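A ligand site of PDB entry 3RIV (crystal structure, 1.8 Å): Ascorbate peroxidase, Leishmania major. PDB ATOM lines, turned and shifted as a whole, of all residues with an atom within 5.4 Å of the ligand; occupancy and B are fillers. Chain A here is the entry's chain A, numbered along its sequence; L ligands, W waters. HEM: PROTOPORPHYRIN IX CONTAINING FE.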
ATOM      1  N   GLU A  25       1.583  28.528 -16.926  1.00  0.00           N
ATOM      2  CA  GLU A  25       1.886  28.749 -15.488  1.00  0.00           C
ATOM      3  C   GLU A  25       0.664  28.479 -14.571  1.00  0.00           C
ATOM      4  O   GLU A  25       0.803  28.304 -13.349  1.00  0.00           O
ATOM      5  CB  GLU A  25       2.475  30.150 -15.262  1.00  0.00           C
ATOM      6  CG  GLU A  25       2.108  31.170 -16.321  1.00  0.00           C
ATOM      7  CD  GLU A  25       2.794  30.908 -17.691  1.00  0.00           C
ATOM      8  OE1 GLU A  25       4.042  30.983 -17.827  1.00  0.00           O
ATOM      9  OE2 GLU A  25       2.026  30.615 -18.642  1.00  0.00           O
ATOM     10  N   PRO A  28       0.777  24.584 -12.590  1.00  0.00           N
ATOM     11  CA  PRO A  28       1.313  24.415 -11.240  1.00  0.00           C
ATOM     12  C   PRO A  28       0.487  25.156 -10.171  1.00  0.00           C
ATOM     13  O   PRO A  28       0.371  24.636  -9.061  1.00  0.00           O
ATOM     14  CB  PRO A  28       2.754  24.992 -11.371  1.00  0.00           C
ATOM     15  CG  PRO A  28       3.097  24.684 -12.830  1.00  0.00           C
ATOM     16  CD  PRO A  28       1.797  25.069 -13.537  1.00  0.00           C
ATOM     17  N   SER A  29      -0.085  26.317 -10.470  1.00  0.00           N
ATOM     18  CA  SER A  29      -0.883  27.002  -9.436  1.00  0.00           C
ATOM     19  C   SER A  29      -2.147  26.227  -9.098  1.00  0.00           C
ATOM     20  O   SER A  29      -2.626  26.304  -7.965  1.00  0.00           O
ATOM     21  CB  SER A  29      -1.232  28.453  -9.783  1.00  0.00           C
ATOM     22  OG  SER A  29      -2.103  28.461 -10.859  1.00  0.00           O
ATOM     23  N   ILE A  31      -2.410  22.925  -9.040  1.00  0.00           N
ATOM     24  CA  ILE A  31      -1.942  21.946  -8.100  1.00  0.00           C
ATOM     25  C   ILE A  31      -1.759  22.523  -6.696  1.00  0.00           C
ATOM     26  O   ILE A  31      -2.201  21.942  -5.721  1.00  0.00           O
ATOM     27  CB  ILE A  31      -0.608  21.277  -8.592  1.00  0.00           C
ATOM     28  CG1 ILE A  31      -0.835  20.604  -9.954  1.00  0.00           C
ATOM     29  CG2 ILE A  31      -0.061  20.307  -7.536  1.00  0.00           C
ATOM     30  CD1 ILE A  31       0.502  20.188 -10.614  1.00  0.00           C
ATOM     31  N   ARG A  32      -1.112  23.687  -6.601  1.00  0.00           N
ATOM     32  CA  ARG A  32      -0.898  24.326  -5.310  1.00  0.00           C
ATOM     33  C   ARG A  32      -2.237  24.667  -4.658  1.00  0.00           C
ATOM     34  O   ARG A  32      -2.395  24.473  -3.447  1.00  0.00           O
ATOM     35  CB  ARG A  32      -0.054  25.616  -5.457  1.00  0.00           C
ATOM     36  CG  ARG A  32       0.328  26.264  -4.088  1.00  0.00           C
ATOM     37  CD  ARG A  32       1.097  27.573  -4.365  1.00  0.00           C
ATOM     38  NE  ARG A  32       1.091  28.400  -3.158  1.00  0.00           N
ATOM     39  CZ  ARG A  32       0.911  29.718  -3.129  1.00  0.00           C
ATOM     40  NH1 ARG A  32       0.712  30.426  -4.249  1.00  0.00           N
ATOM     41  NH2 ARG A  32       0.939  30.332  -1.948  1.00  0.00           N
ATOM     42  N   TRP A  35      -3.830  21.410  -3.268  1.00  0.00           N
ATOM     43  CA  TRP A  35      -3.044  20.992  -2.085  1.00  0.00           C
ATOM     44  C   TRP A  35      -3.313  21.858  -0.857  1.00  0.00           C
ATOM     45  O   TRP A  35      -3.531  21.336   0.243  1.00  0.00           O
ATOM     46  CB  TRP A  35      -1.554  20.878  -2.449  1.00  0.00           C
ATOM     47  CG  TRP A  35      -0.532  21.397  -1.483  1.00  0.00           C
ATOM     48  CD1 TRP A  35       0.328  22.458  -1.689  1.00  0.00           C
ATOM     49  CD2 TRP A  35      -0.151  20.821  -0.207  1.00  0.00           C
ATOM     50  NE1 TRP A  35       1.163  22.610  -0.602  1.00  0.00           N
ATOM     51  CE2 TRP A  35       0.881  21.630   0.319  1.00  0.00           C
ATOM     52  CE3 TRP A  35      -0.611  19.737   0.543  1.00  0.00           C
ATOM     53  CZ2 TRP A  35       1.495  21.363   1.537  1.00  0.00           C
ATOM     54  CZ3 TRP A  35      -0.021  19.480   1.787  1.00  0.00           C
ATOM     55  CH2 TRP A  35       1.032  20.296   2.274  1.00  0.00           C
ATOM     56  N   LYS A  67      -1.201  33.059  -0.157  1.00  0.00           N
ATOM     57  CA  LYS A  67      -1.058  34.231  -1.012  1.00  0.00           C
ATOM     58  C   LYS A  67      -0.815  33.851  -2.483  1.00  0.00           C
ATOM     59  O   LYS A  67       0.003  32.979  -2.784  1.00  0.00           O
ATOM     60  CB  LYS A  67       0.029  35.174  -0.479  1.00  0.00           C
ATOM     61  CG  LYS A  67       0.084  36.536  -1.198  1.00  0.00           C
ATOM     62  CD  LYS A  67       0.991  37.536  -0.415  1.00  0.00           C
ATOM     63  CE  LYS A  67       0.901  38.959  -0.962  1.00  0.00           C
ATOM     64  NZ  LYS A  67       2.161  39.722  -0.673  1.00  0.00           N
ATOM     65  N   PRO A 130       2.494  24.490   5.669  1.00  0.00           N
ATOM     66  CA  PRO A 130       3.909  24.452   6.018  1.00  0.00           C
ATOM     67  C   PRO A 130       4.688  25.725   5.609  1.00  0.00           C
ATOM     68  O   PRO A 130       4.245  26.501   4.752  1.00  0.00           O
ATOM     69  CB  PRO A 130       4.419  23.190   5.312  1.00  0.00           C
ATOM     70  CG  PRO A 130       3.555  23.081   4.117  1.00  0.00           C
ATOM     71  CD  PRO A 130       2.144  23.529   4.604  1.00  0.00           C
ATOM     72  N   ASP A 131       5.817  25.920   6.246  1.00  0.00           N
ATOM     73  CA  ASP A 131       6.598  27.145   6.131  1.00  0.00           C
ATOM     74  C   ASP A 131       7.907  26.740   5.484  1.00  0.00           C
ATOM     75  O   ASP A 131       8.681  25.974   6.064  1.00  0.00           O
ATOM     76  CB  ASP A 131       6.801  27.653   7.565  1.00  0.00           C
ATOM     77  CG  ASP A 131       7.653  28.919   7.668  1.00  0.00           C
ATOM     78  OD1 ASP A 131       8.311  29.340   6.664  1.00  0.00           O
ATOM     79  OD2 ASP A 131       7.649  29.483   8.796  1.00  0.00           O
ATOM     80  N   GLY A 132       8.154  27.213   4.262  1.00  0.00           N
ATOM     81  CA  GLY A 132       9.379  26.865   3.553  1.00  0.00           C
ATOM     82  C   GLY A 132      10.693  27.255   4.211  1.00  0.00           C
ATOM     83  O   GLY A 132      11.732  26.755   3.820  1.00  0.00           O
ATOM     84  N   VAL A 139       8.408  20.067   9.004  1.00  0.00           N
ATOM     85  CA  VAL A 139       7.756  19.342   7.892  1.00  0.00           C
ATOM     86  C   VAL A 139       7.108  18.039   8.441  1.00  0.00           C
ATOM     87  O   VAL A 139       5.991  17.692   8.071  1.00  0.00           O
ATOM     88  CB  VAL A 139       8.771  19.019   6.718  1.00  0.00           C
ATOM     89  CG1 VAL A 139       8.190  17.993   5.694  1.00  0.00           C
ATOM     90  CG2 VAL A 139       9.200  20.350   6.023  1.00  0.00           C
ATOM     91  N   PHE A 143       3.043  17.041   8.263  1.00  0.00           N
ATOM     92  CA  PHE A 143       2.589  15.901   7.522  1.00  0.00           C
ATOM     93  C   PHE A 143       2.031  14.816   8.398  1.00  0.00           C
ATOM     94  O   PHE A 143       1.083  14.158   7.968  1.00  0.00           O
ATOM     95  CB  PHE A 143       3.656  15.429   6.565  1.00  0.00           C
ATOM     96  CG  PHE A 143       3.699  16.262   5.311  1.00  0.00           C
ATOM     97  CD1 PHE A 143       4.377  17.487   5.294  1.00  0.00           C
ATOM     98  CD2 PHE A 143       2.979  15.888   4.206  1.00  0.00           C
ATOM     99  CE1 PHE A 143       4.399  18.277   4.143  1.00  0.00           C
ATOM    100  CE2 PHE A 143       3.009  16.661   3.031  1.00  0.00           C
ATOM    101  CZ  PHE A 143       3.726  17.853   3.013  1.00  0.00           C
ATOM    102  N   LEU A 156       4.879  13.645  -2.060  1.00  0.00           N
ATOM    103  CA  LEU A 156       4.004  14.814  -2.310  1.00  0.00           C
ATOM    104  C   LEU A 156       4.839  16.073  -2.579  1.00  0.00           C
ATOM    105  O   LEU A 156       4.517  16.842  -3.479  1.00  0.00           O
ATOM    106  CB  LEU A 156       3.050  15.081  -1.135  1.00  0.00           C
ATOM    107  CG  LEU A 156       1.873  14.089  -1.034  1.00  0.00           C
ATOM    108  CD1 LEU A 156       1.205  14.191   0.293  1.00  0.00           C
ATOM    109  CD2 LEU A 156       0.833  14.332  -2.152  1.00  0.00           C
ATOM    110  N   ILE A 157       5.897  16.280  -1.784  1.00  0.00           N
ATOM    111  CA  ILE A 157       6.756  17.469  -1.994  1.00  0.00           C
ATOM    112  C   ILE A 157       7.409  17.455  -3.388  1.00  0.00           C
ATOM    113  O   ILE A 157       7.786  18.509  -3.966  1.00  0.00           O
ATOM    114  CB  ILE A 157       7.774  17.652  -0.833  1.00  0.00           C
ATOM    115  CG1 ILE A 157       7.010  17.874   0.464  1.00  0.00           C
ATOM    116  CG2 ILE A 157       8.712  18.868  -1.115  1.00  0.00           C
ATOM    117  CD1 ILE A 157       7.818  17.759   1.765  1.00  0.00           C
ATOM    118  N   ALA A 159       6.014  17.425  -6.030  1.00  0.00           N
ATOM    119  CA  ALA A 159       5.280  18.310  -6.938  1.00  0.00           C
ATOM    120  C   ALA A 159       6.062  19.553  -7.291  1.00  0.00           C
ATOM    121  O   ALA A 159       5.719  20.236  -8.254  1.00  0.00           O
ATOM    122  CB  ALA A 159       3.926  18.722  -6.354  1.00  0.00           C
ATOM    123  N   HIS A 160       7.091  19.880  -6.502  1.00  0.00           N
ATOM    124  CA  HIS A 160       7.928  21.031  -6.817  1.00  0.00           C
ATOM    125  C   HIS A 160       8.736  20.792  -8.087  1.00  0.00           C
ATOM    126  O   HIS A 160       9.461  21.678  -8.560  1.00  0.00           O
ATOM    127  CB  HIS A 160       8.827  21.372  -5.623  1.00  0.00           C
ATOM    128  CG  HIS A 160       8.096  22.009  -4.459  1.00  0.00           C
ATOM    129  ND1 HIS A 160       8.673  22.185  -3.216  1.00  0.00           N
ATOM    130  CD2 HIS A 160       6.853  22.536  -4.382  1.00  0.00           C
ATOM    131  CE1 HIS A 160       7.814  22.793  -2.410  1.00  0.00           C
ATOM    132  NE2 HIS A 160       6.699  23.010  -3.084  1.00  0.00           N
ATOM    133  N   CYS A 162       7.354  20.969 -10.690  1.00  0.00           N
ATOM    134  CA  CYS A 162       6.804  21.974 -11.572  1.00  0.00           C
ATOM    135  C   CYS A 162       6.503  23.286 -10.845  1.00  0.00           C
ATOM    136  O   CYS A 162       6.369  23.335  -9.604  1.00  0.00           O
ATOM    137  CB  CYS A 162       5.571  21.455 -12.305  1.00  0.00           C
ATOM    138  SG  CYS A 162       4.087  21.254 -11.223  1.00  0.00           S
ATOM    139  N   GLY A 163       6.368  24.351 -11.630  1.00  0.00           N
ATOM    140  CA  GLY A 163       6.069  25.675 -11.119  1.00  0.00           C
ATOM    141  C   GLY A 163       7.299  26.372 -10.575  1.00  0.00           C
ATOM    142  O   GLY A 163       8.437  25.940 -10.824  1.00  0.00           O
ATOM    143  N   GLU A 164       7.077  27.432  -9.825  1.00  0.00           N
ATOM    144  CA  GLU A 164       8.140  28.283  -9.348  1.00  0.00           C
ATOM    145  C   GLU A 164       7.660  29.141  -8.225  1.00  0.00           C
ATOM    146  O   GLU A 164       6.470  29.337  -8.050  1.00  0.00           O
ATOM    147  CB  GLU A 164       8.629  29.182 -10.489  1.00  0.00           C
ATOM    148  CG  GLU A 164       7.583  30.137 -11.050  1.00  0.00           C
ATOM    149  CD  GLU A 164       8.035  30.700 -12.407  1.00  0.00           C
ATOM    150  OE1 GLU A 164       7.167  31.037 -13.232  1.00  0.00           O
ATOM    151  OE2 GLU A 164       9.259  30.779 -12.668  1.00  0.00           O
ATOM    152  N   CYS A 165       8.622  29.687  -7.469  1.00  0.00           N
ATOM    153  CA  CYS A 165       8.293  30.649  -6.436  1.00  0.00           C
ATOM    154  C   CYS A 165       8.246  32.072  -6.955  1.00  0.00           C
ATOM    155  O   CYS A 165       8.992  32.434  -7.869  1.00  0.00           O
ATOM    156  CB  CYS A 165       9.320  30.568  -5.312  1.00  0.00           C
ATOM    157  SG  CYS A 165       9.348  28.955  -4.434  1.00  0.00           S
ATOM    158  N   HIS A 166       7.360  32.865  -6.356  1.00  0.00           N
ATOM    159  CA  HIS A 166       7.184  34.275  -6.743  1.00  0.00           C
ATOM    160  C   HIS A 166       7.441  35.167  -5.540  1.00  0.00           C
ATOM    161  O   HIS A 166       6.871  34.943  -4.454  1.00  0.00           O
ATOM    162  CB  HIS A 166       5.754  34.537  -7.249  1.00  0.00           C
ATOM    163  CG  HIS A 166       5.294  33.566  -8.280  1.00  0.00           C
ATOM    164  ND1 HIS A 166       4.636  32.391  -7.963  1.00  0.00           N
ATOM    165  CD2 HIS A 166       5.401  33.584  -9.638  1.00  0.00           C
ATOM    166  CE1 HIS A 166       4.370  31.728  -9.066  1.00  0.00           C
ATOM    167  NE2 HIS A 166       4.824  32.433 -10.097  1.00  0.00           N
ATOM    168  N   ILE A 167       8.277  36.204  -5.720  1.00  0.00           N
ATOM    169  CA  ILE A 167       8.651  37.054  -4.590  1.00  0.00           C
ATOM    170  C   ILE A 167       7.398  37.675  -3.962  1.00  0.00           C
ATOM    171  O   ILE A 167       7.290  37.730  -2.733  1.00  0.00           O
ATOM    172  CB  ILE A 167       9.720  38.155  -4.985  1.00  0.00           C
ATOM    173  CG1 ILE A 167      11.070  37.512  -5.357  1.00  0.00           C
ATOM    174  CG2 ILE A 167       9.923  39.185  -3.847  1.00  0.00           C
ATOM    175  CD1 ILE A 167      11.882  36.956  -4.197  1.00  0.00           C
ATOM    176  N   PHE A 169       4.465  36.500  -3.642  1.00  0.00           N
ATOM    177  CA  PHE A 169       3.571  35.562  -2.923  1.00  0.00           C
ATOM    178  C   PHE A 169       4.234  34.943  -1.679  1.00  0.00           C
ATOM    179  O   PHE A 169       3.680  34.939  -0.584  1.00  0.00           O
ATOM    180  CB  PHE A 169       3.050  34.431  -3.839  1.00  0.00           C
ATOM    181  CG  PHE A 169       2.281  34.902  -5.052  1.00  0.00           C
ATOM    182  CD1 PHE A 169       1.630  36.151  -5.068  1.00  0.00           C
ATOM    183  CD2 PHE A 169       2.166  34.070  -6.173  1.00  0.00           C
ATOM    184  CE1 PHE A 169       0.923  36.564  -6.201  1.00  0.00           C
ATOM    185  CE2 PHE A 169       1.465  34.471  -7.299  1.00  0.00           C
ATOM    186  CZ  PHE A 169       0.835  35.732  -7.312  1.00  0.00           C
ATOM    187  N   SER A 170       5.423  34.376  -1.833  1.00  0.00           N
ATOM    188  CA  SER A 170       6.086  33.692  -0.735  1.00  0.00           C
ATOM    189  C   SER A 170       7.373  34.370  -0.266  1.00  0.00           C
ATOM    190  O   SER A 170       7.870  34.029   0.799  1.00  0.00           O
ATOM    191  CB  SER A 170       6.435  32.251  -1.150  1.00  0.00           C
ATOM    192  OG  SER A 170       7.358  32.258  -2.248  1.00  0.00           O
ATOM    193  N   GLY A 171       7.927  35.256  -1.103  1.00  0.00           N
ATOM    194  CA  GLY A 171       9.213  35.899  -0.822  1.00  0.00           C
ATOM    195  C   GLY A 171      10.387  35.087  -1.325  1.00  0.00           C
ATOM    196  O   GLY A 171      11.542  35.482  -1.169  1.00  0.00           O
ATOM    197  N   TYR A 172      10.097  33.953  -1.938  1.00  0.00           N
ATOM    198  CA  TYR A 172      11.135  33.189  -2.608  1.00  0.00           C
ATOM    199  C   TYR A 172      11.063  33.420  -4.107  1.00  0.00           C
ATOM    200  O   TYR A 172      10.098  34.005  -4.605  1.00  0.00           O
ATOM    201  CB  TYR A 172      10.981  31.720  -2.261  1.00  0.00           C
ATOM    202  CG  TYR A 172      11.194  31.407  -0.819  1.00  0.00           C
ATOM    203  CD1 TYR A 172      12.465  31.400  -0.256  1.00  0.00           C
ATOM    204  CD2 TYR A 172      10.110  31.097   0.007  1.00  0.00           C
ATOM    205  CE1 TYR A 172      12.670  31.119   1.102  1.00  0.00           C
ATOM    206  CE2 TYR A 172      10.296  30.792   1.354  1.00  0.00           C
ATOM    207  CZ  TYR A 172      11.589  30.793   1.877  1.00  0.00           C
ATOM    208  OH  TYR A 172      11.770  30.500   3.218  1.00  0.00           O
ATOM    209  N   TRP A 176      12.308  25.176  -9.393  1.00  0.00           N
ATOM    210  CA  TRP A 176      13.134  24.129  -8.822  1.00  0.00           C
ATOM    211  C   TRP A 176      13.898  23.288  -9.860  1.00  0.00           C
ATOM    212  O   TRP A 176      14.870  22.598  -9.524  1.00  0.00           O
ATOM    213  CB  TRP A 176      12.251  23.149  -8.027  1.00  0.00           C
ATOM    214  CG  TRP A 176      11.674  23.694  -6.764  1.00  0.00           C
ATOM    215  CD1 TRP A 176      12.230  23.604  -5.517  1.00  0.00           C
ATOM    216  CD2 TRP A 176      10.425  24.403  -6.595  1.00  0.00           C
ATOM    217  NE1 TRP A 176      11.427  24.222  -4.591  1.00  0.00           N
ATOM    218  CE2 TRP A 176      10.302  24.696  -5.206  1.00  0.00           C
ATOM    219  CE3 TRP A 176       9.407  24.790  -7.484  1.00  0.00           C
ATOM    220  CZ2 TRP A 176       9.193  25.393  -4.668  1.00  0.00           C
ATOM    221  CZ3 TRP A 176       8.262  25.485  -6.933  1.00  0.00           C
ATOM    222  CH2 TRP A 176       8.193  25.785  -5.546  1.00  0.00           C
ATOM    223  N   LEU A 218      14.273  25.387  -1.350  1.00  0.00           N
ATOM    224  CA  LEU A 218      13.923  26.012  -0.076  1.00  0.00           C
ATOM    225  C   LEU A 218      14.594  25.224   1.047  1.00  0.00           C
ATOM    226  O   LEU A 218      14.962  24.060   0.822  1.00  0.00           O
ATOM    227  CB  LEU A 218      12.406  25.910   0.144  1.00  0.00           C
ATOM    228  CG  LEU A 218      11.398  26.525  -0.849  1.00  0.00           C
ATOM    229  CD1 LEU A 218      10.027  25.925  -0.660  1.00  0.00           C
ATOM    230  CD2 LEU A 218      11.368  28.011  -0.701  1.00  0.00           C
ATOM    231  N   SER A 220      13.018  23.899   3.386  1.00  0.00           N
ATOM    232  CA  SER A 220      12.104  22.751   3.557  1.00  0.00           C
ATOM    233  C   SER A 220      12.303  21.665   2.473  1.00  0.00           C
ATOM    234  O   SER A 220      11.977  20.495   2.722  1.00  0.00           O
ATOM    235  CB  SER A 220      10.645  23.264   3.522  1.00  0.00           C
ATOM    236  OG  SER A 220      10.436  23.889   2.266  1.00  0.00           O
ATOM    237  N   PHE A 248       3.269   9.227  -6.046  1.00  0.00           N
ATOM    238  CA  PHE A 248       2.641  10.546  -6.064  1.00  0.00           C
ATOM    239  C   PHE A 248       1.137  10.447  -6.328  1.00  0.00           C
ATOM    240  O   PHE A 248       0.347  11.142  -5.655  1.00  0.00           O
ATOM    241  CB  PHE A 248       3.309  11.515  -7.035  1.00  0.00           C
ATOM    242  CG  PHE A 248       2.673  12.885  -7.015  1.00  0.00           C
ATOM    243  CD1 PHE A 248       3.131  13.842  -6.128  1.00  0.00           C
ATOM    244  CD2 PHE A 248       1.555  13.157  -7.830  1.00  0.00           C
ATOM    245  CE1 PHE A 248       2.517  15.108  -6.078  1.00  0.00           C
ATOM    246  CE2 PHE A 248       0.925  14.382  -7.779  1.00  0.00           C
ATOM    247  CZ  PHE A 248       1.388  15.369  -6.906  1.00  0.00           C
ATOM    248  N   PHE A 252      -1.417  11.866  -3.592  1.00  0.00           N
ATOM    249  CA  PHE A 252      -2.187  13.058  -3.947  1.00  0.00           C
ATOM    250  C   PHE A 252      -3.669  12.773  -3.968  1.00  0.00           C
ATOM    251  O   PHE A 252      -4.493  13.649  -3.586  1.00  0.00           O
ATOM    252  CB  PHE A 252      -1.712  13.627  -5.266  1.00  0.00           C
ATOM    253  CG  PHE A 252      -2.180  15.021  -5.528  1.00  0.00           C
ATOM    254  CD1 PHE A 252      -1.566  16.116  -4.875  1.00  0.00           C
ATOM    255  CD2 PHE A 252      -3.254  15.267  -6.402  1.00  0.00           C
ATOM    256  CE1 PHE A 252      -2.019  17.411  -5.092  1.00  0.00           C
ATOM    257  CE2 PHE A 252      -3.712  16.562  -6.647  1.00  0.00           C
ATOM    258  CZ  PHE A 252      -3.098  17.668  -5.972  1.00  0.00           C
ATOM    259  N   LEU A 255      -4.518  12.747  -0.308  1.00  0.00           N
ATOM    260  CA  LEU A 255      -4.594  14.144   0.098  1.00  0.00           C
ATOM    261  C   LEU A 255      -5.934  14.819  -0.257  1.00  0.00           C
ATOM    262  O   LEU A 255      -6.535  15.485   0.604  1.00  0.00           O
ATOM    263  CB  LEU A 255      -3.445  14.919  -0.571  1.00  0.00           C
ATOM    264  CG  LEU A 255      -3.374  16.410  -0.304  1.00  0.00           C
ATOM    265  CD1 LEU A 255      -2.889  16.758   1.125  1.00  0.00           C
ATOM    266  CD2 LEU A 255      -2.426  17.087  -1.334  1.00  0.00           C
HETATM  267  CHA HEM L   1       4.847  26.489  -4.587  1.00  0.00           C
HETATM  268  CHB HEM L   1       6.319  25.619  -0.054  1.00  0.00           C
HETATM  269  CHC HEM L   1       4.593  21.117  -0.308  1.00  0.00           C
HETATM  270  CHD HEM L   1       2.846  22.065  -4.767  1.00  0.00           C
HETATM  271  C1A HEM L   1       5.370  26.652  -3.321  1.00  0.00           C
HETATM  272  C2A HEM L   1       5.988  27.872  -2.831  1.00  0.00           C
HETATM  273  C3A HEM L   1       6.409  27.651  -1.576  1.00  0.00           C
HETATM  274  C4A HEM L   1       6.061  26.275  -1.235  1.00  0.00           C
HETATM  275  CMA HEM L   1       7.138  28.655  -0.652  1.00  0.00           C
HETATM  276  CAA HEM L   1       6.083  29.181  -3.659  1.00  0.00           C
HETATM  277  CBA HEM L   1       4.700  29.846  -3.705  1.00  0.00           C
HETATM  278  CGA HEM L   1       4.787  31.076  -4.613  1.00  0.00           C
HETATM  279  O1A HEM L   1       5.636  31.966  -4.296  1.00  0.00           O
HETATM  280  O2A HEM L   1       4.035  31.183  -5.608  1.00  0.00           O
HETATM  281  C1B HEM L   1       6.025  24.325   0.280  1.00  0.00           C
HETATM  282  C2B HEM L   1       6.355  23.652   1.512  1.00  0.00           C
HETATM  283  C3B HEM L   1       5.836  22.416   1.442  1.00  0.00           C
HETATM  284  C4B HEM L   1       5.224  22.258   0.149  1.00  0.00           C
HETATM  285  CMB HEM L   1       7.076  24.289   2.710  1.00  0.00           C
HETATM  286  CAB HEM L   1       5.973  21.281   2.476  1.00  0.00           C
HETATM  287  CBB HEM L   1       7.117  21.168   3.190  1.00  0.00           C
HETATM  288  C1C HEM L   1       3.900  21.029  -1.519  1.00  0.00           C
HETATM  289  C2C HEM L   1       3.018  19.949  -1.907  1.00  0.00           C
HETATM  290  C3C HEM L   1       2.531  20.225  -3.127  1.00  0.00           C
HETATM  291  C4C HEM L   1       3.086  21.493  -3.537  1.00  0.00           C
HETATM  292  CMC HEM L   1       2.736  18.738  -0.998  1.00  0.00           C
HETATM  293  CAC HEM L   1       1.551  19.393  -3.986  1.00  0.00           C
HETATM  294  CBC HEM L   1       1.412  18.075  -3.898  1.00  0.00           C
HETATM  295  C1D HEM L   1       3.324  23.290  -5.172  1.00  0.00           C
HETATM  296  C2D HEM L   1       3.345  23.745  -6.539  1.00  0.00           C
HETATM  297  C3D HEM L   1       3.966  25.099  -6.486  1.00  0.00           C
HETATM  298  C4D HEM L   1       4.289  25.346  -5.101  1.00  0.00           C
HETATM  299  CMD HEM L   1       2.858  23.017  -7.797  1.00  0.00           C
HETATM  300  CAD HEM L   1       4.221  26.018  -7.705  1.00  0.00           C
HETATM  301  CBD HEM L   1       3.067  27.036  -7.734  1.00  0.00           C
HETATM  302  CGD HEM L   1       3.163  27.967  -8.931  1.00  0.00           C
HETATM  303  O1D HEM L   1       2.336  28.919  -9.008  1.00  0.00           O
HETATM  304  O2D HEM L   1       4.002  27.771  -9.824  1.00  0.00           O
HETATM  305  NA  HEM L   1       5.480  25.691  -2.342  1.00  0.00           N
HETATM  306  NB  HEM L   1       5.367  23.430  -0.533  1.00  0.00           N
HETATM  307  NC  HEM L   1       3.922  21.949  -2.552  1.00  0.00           N
HETATM  308  ND  HEM L   1       3.947  24.242  -4.366  1.00  0.00           N
HETATM  309 FE   HEM L   1       4.785  23.776  -2.460  1.00  0.00          FE
HETATM  310  O   HOH W   1       2.922  24.794   0.987  1.00  0.00           O
HETATM  311  O   HOH W   2       1.461  30.232  -6.751  1.00  0.00           O
HETATM  312  O   HOH W   3       3.047  24.642  -1.723  1.00  0.00           O
HETATM  313  O   HOH W   4       2.865  27.614  -0.936  1.00  0.00           O
HETATM  314  O   HOH W   5       3.588  28.546 -12.305  1.00  0.00           O
HETATM  315  O   HOH W   6       1.927  30.527 -11.095  1.00  0.00           O
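FE of the ligand is bound by NE2 of His 160, at 2.2 Å.
O1A of the ligand sits close to N of Ser 170, at 3.5 Å.
OG of Ser 170 is in hydrogen-bond range of O1A of the ligand, at 2.7 Å.
O1A of the ligand is in hydrogen-bond range of N of His 166 (2.8 Å).
ND1 of His 166 sits at hydrogen-bond distance from O2A of the ligand.
N of Glu 164 lies within hydrogen-bond range of O2D of the ligand (3.1 Å).
O2A of the ligand is in salt-bridge range of NH1 of Arg 32, at 3.7 Å.
The side-chain hydroxyl (OG) of Ser 170 lies close to the backbone NH (N) of Tyr 172, 3.2 Å away.
N of His 166 sits close to O of Tyr 172 (3.4 Å).
The backbone carbonyl oxygen of Gly 132 is in hydrogen-bond range of the backbone NH of Ser 220 (3.2 Å).
SG of Cys 162 sits at hydrogen-bond distance from O of Ala 159, 3.5 Å away.
NH2 of Arg 32 is in hydrogen-bond range of O of Lys 67.
The backbone carbonyl oxygen of Tyr 172 sits at hydrogen-bond distance from the backbone NH of Ile 167, 3.1 Å away.
NE1 of Trp 35 lies close to NC of the ligand, 3.4 Å away.
Merely in contact with the ligand: Pro 28, Ser 29, Ile 31, Pro 130, Asp 131, Gly 132, Val 139, Phe 143, Leu 156, Ile 157, Ala 159, Cys 162, Gly 163, Cys 165, Phe 169, Tyr 172, Trp 176, Leu 218, Ser 220, Phe 248 and Phe 252.
Hydrophobic or aromatic side chains within 4 Å of the ligand: Pro 28, Ile 31, Trp 35, Pro 130, Val 139, Phe 143, Leu 156, Ile 157, Ala 159, His 160, His 166, Phe 169, Tyr 172, Trp 176, Leu 218, Phe 248 and Phe 252.
Water W5 bridges an oxygen (O2D) of the ligand (2.6 Å) and the backbone carbonyl oxygen of Glu 25 (3.0 Å).
Water W6 bridges an oxygen (O1D) of the ligand and the backbone carbonyl oxygen of Glu 25.
Water W2 bridges NH1 of Arg 32 and O1D of the ligand.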
